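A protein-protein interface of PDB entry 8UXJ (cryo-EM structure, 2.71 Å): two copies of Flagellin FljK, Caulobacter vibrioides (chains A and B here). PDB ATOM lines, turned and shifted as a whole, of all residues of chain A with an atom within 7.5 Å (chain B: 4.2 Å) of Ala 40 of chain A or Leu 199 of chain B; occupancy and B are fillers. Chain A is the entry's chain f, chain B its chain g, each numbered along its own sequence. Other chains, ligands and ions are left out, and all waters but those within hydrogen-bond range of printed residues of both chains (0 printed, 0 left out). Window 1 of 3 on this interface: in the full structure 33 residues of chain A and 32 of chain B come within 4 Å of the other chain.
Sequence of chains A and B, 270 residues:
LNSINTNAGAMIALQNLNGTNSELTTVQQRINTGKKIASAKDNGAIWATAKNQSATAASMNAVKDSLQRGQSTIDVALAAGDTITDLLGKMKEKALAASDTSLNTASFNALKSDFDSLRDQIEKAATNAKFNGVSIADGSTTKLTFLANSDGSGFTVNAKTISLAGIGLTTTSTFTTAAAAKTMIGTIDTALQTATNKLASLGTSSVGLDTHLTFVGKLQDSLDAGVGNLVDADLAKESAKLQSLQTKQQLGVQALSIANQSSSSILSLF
Of the printed residues of chain B, Gly 44 of chain A touches Ala 200.
Printed residues of chain B within 4 Å of Trp 47 of chain A: Thr 196, Leu 199 and Ala 200.
Of the printed residues of chain B, Ala 48 of chain A touches Thr 196 (3.98 Å).
Leu 78 of chain B touches none of the printed residues of chain A.
Printed residues of chain A within 4 Å of Gly 203 of chain B: Ala 40.
The nearest residue of chain A that does not touch Leu 199 of chain B is Gly 44 of chain A (6.1 Å).
The nearest printed residue of chain A that does not touch Thr 196 of chain B is Lys 51 of chain A (4.3 Å).
Of the 12 printed residues of chain A, 4 touch a printed residue of chain B.
Printed residues of chain A that touch a printed residue of chain B: Ala 40, Gly 44, Trp 47 and Ala 48.
Hydrophobic or aromatic side chains of chain A within 4 Å of the printed part of chain B: Ala 40, Trp 47 and Ala 48.
Along chain A the printed residues that touch a printed residue of chain B span positions 40 to 48.
Hydrophobic or aromatic side chains of chain B that line the printed part of chain A: Leu 199 and Ala 200.
Among the printed residues, 8 pairs touch across the chains.
Among the printed residues, no Asp or Glu carboxylate lies within 4 Å of a Lys or Arg side-chain nitrogen of the other chain.
Among the printed residues, merely in contact across the chains: Gly 44 of chain A with Ala 200 of chain B (3.4 Å), Trp 47 of chain A with Thr 196 of chain B (3.5 Å), Ala 40 of chain A with Leu 199 of chain B (3.6 Å), Ala 40 of chain A with Gly 203 of chain B (3.7 Å), Trp 47 of chain A with Leu 199 of chain B (3.8 Å), Trp 47 of chain A with Ala 200 of chain B (3.8 Å), Ala 40 of chain A with Ala 200 of chain B (3.9 Å) and Ala 48 of chain A with Thr 196 of chain B (3.98 Å).
No position is printed for both chains.
Of the 8 pairs that touch across the chains among the printed residues, none has its exchanged pair printed and touching as well.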
ATOM      1  N   ILE A  37     -25.521   5.918  -3.050  1.00  0.00           N
ATOM      2  CA  ILE A  37     -25.364   7.291  -2.585  1.00  0.00           C
ATOM      3  C   ILE A  37     -24.173   7.300  -1.637  1.00  0.00           C
ATOM      4  O   ILE A  37     -24.331   7.274  -0.410  1.00  0.00           O
ATOM      5  CB  ILE A  37     -26.646   7.817  -1.917  1.00  0.00           C
ATOM      6  CG1 ILE A  37     -27.787   7.848  -2.930  1.00  0.00           C
ATOM      7  CG2 ILE A  37     -26.441   9.228  -1.396  1.00  0.00           C
ATOM      8  CD1 ILE A  37     -29.138   8.102  -2.313  1.00  0.00           C
ATOM      9  N   ALA A  38     -22.967   7.292  -2.207  1.00  0.00           N
ATOM     10  CA  ALA A  38     -21.760   7.227  -1.394  1.00  0.00           C
ATOM     11  C   ALA A  38     -21.500   8.532  -0.659  1.00  0.00           C
ATOM     12  O   ALA A  38     -20.869   8.527   0.404  1.00  0.00           O
ATOM     13  CB  ALA A  38     -20.559   6.867  -2.268  1.00  0.00           C
ATOM     14  N   SER A  39     -21.969   9.651  -1.200  1.00  0.00           N
ATOM     15  CA  SER A  39     -21.657  10.957  -0.638  1.00  0.00           C
ATOM     16  C   SER A  39     -22.669  11.967  -1.160  1.00  0.00           C
ATOM     17  O   SER A  39     -23.566  11.634  -1.938  1.00  0.00           O
ATOM     18  CB  SER A  39     -20.226  11.372  -0.987  1.00  0.00           C
ATOM     19  OG  SER A  39     -20.025  11.353  -2.389  1.00  0.00           O
ATOM     20  N   ALA A  40     -22.509  13.217  -0.723  1.00  0.00           N
ATOM     21  CA  ALA A  40     -23.336  14.304  -1.231  1.00  0.00           C
ATOM     22  C   ALA A  40     -23.116  14.544  -2.717  1.00  0.00           C
ATOM     23  O   ALA A  40     -23.925  15.228  -3.350  1.00  0.00           O
ATOM     24  CB  ALA A  40     -23.057  15.585  -0.449  1.00  0.00           C
ATOM     25  N   LYS A  41     -22.030  14.010  -3.279  1.00  0.00           N
ATOM     26  CA  LYS A  41     -21.767  14.167  -4.704  1.00  0.00           C
ATOM     27  C   LYS A  41     -22.844  13.506  -5.556  1.00  0.00           C
ATOM     28  O   LYS A  41     -23.171  14.003  -6.638  1.00  0.00           O
ATOM     29  CB  LYS A  41     -20.392  13.588  -5.039  1.00  0.00           C
ATOM     30  CG  LYS A  41     -19.879  13.896  -6.435  1.00  0.00           C
ATOM     31  CD  LYS A  41     -19.873  15.385  -6.718  1.00  0.00           C
ATOM     32  CE  LYS A  41     -18.690  15.771  -7.593  1.00  0.00           C
ATOM     33  NZ  LYS A  41     -18.607  14.956  -8.834  1.00  0.00           N
ATOM     34  N   ASP A  42     -23.408  12.392  -5.089  1.00  0.00           N
ATOM     35  CA  ASP A  42     -24.397  11.666  -5.875  1.00  0.00           C
ATOM     36  C   ASP A  42     -25.817  12.166  -5.641  1.00  0.00           C
ATOM     37  O   ASP A  42     -26.586  12.307  -6.598  1.00  0.00           O
ATOM     38  CB  ASP A  42     -24.315  10.170  -5.565  1.00  0.00           C
ATOM     39  CG  ASP A  42     -22.922   9.611  -5.772  1.00  0.00           C
ATOM     40  OD1 ASP A  42     -22.492   8.765  -4.961  1.00  0.00           O
ATOM     41  OD2 ASP A  42     -22.255  10.018  -6.746  1.00  0.00           O
ATOM     42  N   ASN A  43     -26.184  12.440  -4.390  1.00  0.00           N
ATOM     43  CA  ASN A  43     -27.533  12.895  -4.080  1.00  0.00           C
ATOM     44  C   ASN A  43     -27.517  13.524  -2.691  1.00  0.00           C
ATOM     45  O   ASN A  43     -27.431  12.814  -1.687  1.00  0.00           O
ATOM     46  CB  ASN A  43     -28.512  11.716  -4.183  1.00  0.00           C
ATOM     47  CG  ASN A  43     -29.896  12.022  -3.631  1.00  0.00           C
ATOM     48  OD1 ASN A  43     -30.058  12.593  -2.554  1.00  0.00           O
ATOM     49  ND2 ASN A  43     -30.913  11.637  -4.391  1.00  0.00           N
ATOM     50  N   GLY A  44     -27.603  14.854  -2.626  1.00  0.00           N
ATOM     51  CA  GLY A  44     -27.339  15.544  -1.372  1.00  0.00           C
ATOM     52  C   GLY A  44     -28.392  15.319  -0.303  1.00  0.00           C
ATOM     53  O   GLY A  44     -28.061  15.117   0.869  1.00  0.00           O
ATOM     54  N   ALA A  45     -29.671  15.349  -0.683  1.00  0.00           N
ATOM     55  CA  ALA A  45     -30.737  15.352   0.318  1.00  0.00           C
ATOM     56  C   ALA A  45     -30.844  14.007   1.030  1.00  0.00           C
ATOM     57  O   ALA A  45     -30.855  13.945   2.268  1.00  0.00           O
ATOM     58  CB  ALA A  45     -32.064  15.722  -0.339  1.00  0.00           C
ATOM     59  N   TRP A  47     -28.556  11.727   1.092  1.00  0.00           N
ATOM     60  CA  TRP A  47     -27.304  11.505   1.809  1.00  0.00           C
ATOM     61  C   TRP A  47     -27.317  12.192   3.170  1.00  0.00           C
ATOM     62  O   TRP A  47     -26.882  11.609   4.171  1.00  0.00           O
ATOM     63  CB  TRP A  47     -26.123  12.005   0.980  1.00  0.00           C
ATOM     64  CG  TRP A  47     -24.852  12.112   1.759  1.00  0.00           C
ATOM     65  CD1 TRP A  47     -23.957  11.115   1.999  1.00  0.00           C
ATOM     66  CD2 TRP A  47     -24.343  13.277   2.419  1.00  0.00           C
ATOM     67  NE1 TRP A  47     -22.913  11.588   2.753  1.00  0.00           N
ATOM     68  CE2 TRP A  47     -23.129  12.911   3.030  1.00  0.00           C
ATOM     69  CE3 TRP A  47     -24.794  14.592   2.551  1.00  0.00           C
ATOM     70  CZ2 TRP A  47     -22.361  13.811   3.760  1.00  0.00           C
ATOM     71  CZ3 TRP A  47     -24.029  15.486   3.275  1.00  0.00           C
ATOM     72  CH2 TRP A  47     -22.827  15.092   3.871  1.00  0.00           C
ATOM     73  N   ALA A  48     -27.811  13.431   3.223  1.00  0.00           N
ATOM     74  CA  ALA A  48     -27.880  14.145   4.493  1.00  0.00           C
ATOM     75  C   ALA A  48     -28.838  13.461   5.458  1.00  0.00           C
ATOM     76  O   ALA A  48     -28.527  13.299   6.647  1.00  0.00           O
ATOM     77  CB  ALA A  48     -28.304  15.593   4.254  1.00  0.00           C
ATOM     78  N   LYS A  51     -27.110  10.349   6.814  1.00  0.00           N
ATOM     79  CA  LYS A  51     -26.163  10.648   7.886  1.00  0.00           C
ATOM     80  C   LYS A  51     -26.881  10.966   9.190  1.00  0.00           C
ATOM     81  O   LYS A  51     -26.480  10.489  10.262  1.00  0.00           O
ATOM     82  CB  LYS A  51     -25.239  11.798   7.486  1.00  0.00           C
ATOM     83  CG  LYS A  51     -24.372  11.503   6.283  1.00  0.00           C
ATOM     84  CD  LYS A  51     -23.367  10.419   6.648  1.00  0.00           C
ATOM     85  CE  LYS A  51     -22.408  10.123   5.517  1.00  0.00           C
ATOM     86  NZ  LYS A  51     -21.461   9.034   5.869  1.00  0.00           N
ATOM     87  N   LEU B  78     -15.374  18.670   0.718  1.00  0.00           N
ATOM     88  CA  LEU B  78     -16.212  17.543   1.122  1.00  0.00           C
ATOM     89  C   LEU B  78     -15.399  16.463   1.821  1.00  0.00           C
ATOM     90  O   LEU B  78     -15.906  15.787   2.727  1.00  0.00           O
ATOM     91  CB  LEU B  78     -16.959  16.966  -0.080  1.00  0.00           C
ATOM     92  CG  LEU B  78     -17.762  17.963  -0.915  1.00  0.00           C
ATOM     93  CD1 LEU B  78     -18.139  17.382  -2.270  1.00  0.00           C
ATOM     94  CD2 LEU B  78     -18.991  18.419  -0.151  1.00  0.00           C
ATOM     95  N   GLY B  81     -15.402  17.625   5.116  1.00  0.00           N
ATOM     96  CA  GLY B  81     -16.732  17.734   5.696  1.00  0.00           C
ATOM     97  C   GLY B  81     -17.319  16.409   6.143  1.00  0.00           C
ATOM     98  O   GLY B  81     -17.978  16.335   7.181  1.00  0.00           O
ATOM     99  N   THR B  85     -18.664  15.459   9.842  1.00  0.00           N
ATOM    100  CA  THR B  85     -19.957  14.908  10.244  1.00  0.00           C
ATOM    101  C   THR B  85     -19.790  13.615  11.027  1.00  0.00           C
ATOM    102  O   THR B  85     -20.533  13.366  11.983  1.00  0.00           O
ATOM    103  CB  THR B  85     -20.860  14.674   9.037  1.00  0.00           C
ATOM    104  OG1 THR B  85     -20.434  13.498   8.333  1.00  0.00           O
ATOM    105  CG2 THR B  85     -20.870  15.877   8.122  1.00  0.00           C
ATOM    106  N   ALA B 195     -24.545  21.123   9.525  1.00  0.00           N
ATOM    107  CA  ALA B 195     -23.373  20.698   8.765  1.00  0.00           C
ATOM    108  C   ALA B 195     -23.766  19.819   7.581  1.00  0.00           C
ATOM    109  O   ALA B 195     -23.251  19.993   6.464  1.00  0.00           O
ATOM    110  CB  ALA B 195     -22.395  19.962   9.678  1.00  0.00           C
ATOM    111  N   THR B 196     -24.679  18.867   7.805  1.00  0.00           N
ATOM    112  CA  THR B 196     -25.090  17.981   6.719  1.00  0.00           C
ATOM    113  C   THR B 196     -25.762  18.759   5.597  1.00  0.00           C
ATOM    114  O   THR B 196     -25.512  18.492   4.414  1.00  0.00           O
ATOM    115  CB  THR B 196     -26.015  16.883   7.242  1.00  0.00           C
ATOM    116  OG1 THR B 196     -27.196  17.471   7.799  1.00  0.00           O
ATOM    117  CG2 THR B 196     -25.309  16.038   8.285  1.00  0.00           C
ATOM    118  N   ASN B 197     -26.614  19.729   5.940  1.00  0.00           N
ATOM    119  CA  ASN B 197     -27.263  20.510   4.890  1.00  0.00           C
ATOM    120  C   ASN B 197     -26.245  21.305   4.078  1.00  0.00           C
ATOM    121  O   ASN B 197     -26.325  21.354   2.839  1.00  0.00           O
ATOM    122  CB  ASN B 197     -28.316  21.437   5.496  1.00  0.00           C
ATOM    123  CG  ASN B 197     -29.496  20.679   6.058  1.00  0.00           C
ATOM    124  OD1 ASN B 197     -29.996  19.741   5.436  1.00  0.00           O
ATOM    125  ND2 ASN B 197     -29.952  21.080   7.237  1.00  0.00           N
ATOM    126  N   LYS B 198     -25.269  21.925   4.752  1.00  0.00           N
ATOM    127  CA  LYS B 198     -24.272  22.703   4.017  1.00  0.00           C
ATOM    128  C   LYS B 198     -23.466  21.824   3.066  1.00  0.00           C
ATOM    129  O   LYS B 198     -23.224  22.201   1.909  1.00  0.00           O
ATOM    130  CB  LYS B 198     -23.349  23.438   4.988  1.00  0.00           C
ATOM    131  CG  LYS B 198     -24.082  24.369   5.939  1.00  0.00           C
ATOM    132  CD  LYS B 198     -23.197  24.822   7.084  1.00  0.00           C
ATOM    133  CE  LYS B 198     -22.652  26.216   6.832  1.00  0.00           C
ATOM    134  NZ  LYS B 198     -23.732  27.233   6.754  1.00  0.00           N
ATOM    135  N   LEU B 199     -23.056  20.640   3.524  1.00  0.00           N
ATOM    136  CA  LEU B 199     -22.283  19.768   2.642  1.00  0.00           C
ATOM    137  C   LEU B 199     -23.126  19.234   1.485  1.00  0.00           C
ATOM    138  O   LEU B 199     -22.613  19.047   0.373  1.00  0.00           O
ATOM    139  CB  LEU B 199     -21.647  18.631   3.435  1.00  0.00           C
ATOM    140  CG  LEU B 199     -20.614  19.149   4.435  1.00  0.00           C
ATOM    141  CD1 LEU B 199     -20.376  18.161   5.545  1.00  0.00           C
ATOM    142  CD2 LEU B 199     -19.315  19.480   3.720  1.00  0.00           C
ATOM    143  N   ALA B 200     -24.418  18.981   1.719  1.00  0.00           N
ATOM    144  CA  ALA B 200     -25.284  18.573   0.614  1.00  0.00           C
ATOM    145  C   ALA B 200     -25.360  19.660  -0.455  1.00  0.00           C
ATOM    146  O   ALA B 200     -25.280  19.374  -1.663  1.00  0.00           O
ATOM    147  CB  ALA B 200     -26.677  18.232   1.141  1.00  0.00           C
ATOM    148  N   SER B 201     -25.491  20.919  -0.028  1.00  0.00           N
ATOM    149  CA  SER B 201     -25.497  22.018  -0.990  1.00  0.00           C
ATOM    150  C   SER B 201     -24.172  22.097  -1.742  1.00  0.00           C
ATOM    151  O   SER B 201     -24.145  22.364  -2.954  1.00  0.00           O
ATOM    152  CB  SER B 201     -25.791  23.336  -0.278  1.00  0.00           C
ATOM    153  OG  SER B 201     -25.621  24.436  -1.152  1.00  0.00           O
ATOM    154  N   LEU B 202     -23.060  21.868  -1.039  1.00  0.00           N
ATOM    155  CA  LEU B 202     -21.755  21.866  -1.700  1.00  0.00           C
ATOM    156  C   LEU B 202     -21.678  20.793  -2.782  1.00  0.00           C
ATOM    157  O   LEU B 202     -21.161  21.038  -3.883  1.00  0.00           O
ATOM    158  CB  LEU B 202     -20.650  21.661  -0.666  1.00  0.00           C
ATOM    159  CG  LEU B 202     -20.307  22.905   0.147  1.00  0.00           C
ATOM    160  CD1 LEU B 202     -19.360  22.572   1.290  1.00  0.00           C
ATOM    161  CD2 LEU B 202     -19.717  23.953  -0.767  1.00  0.00           C
ATOM    162  N   GLY B 203     -22.184  19.598  -2.484  1.00  0.00           N
ATOM    163  CA  GLY B 203     -22.179  18.539  -3.482  1.00  0.00           C
ATOM    164  C   GLY B 203     -22.993  18.896  -4.712  1.00  0.00           C
ATOM    165  O   GLY B 203     -22.562  18.657  -5.849  1.00  0.00           O
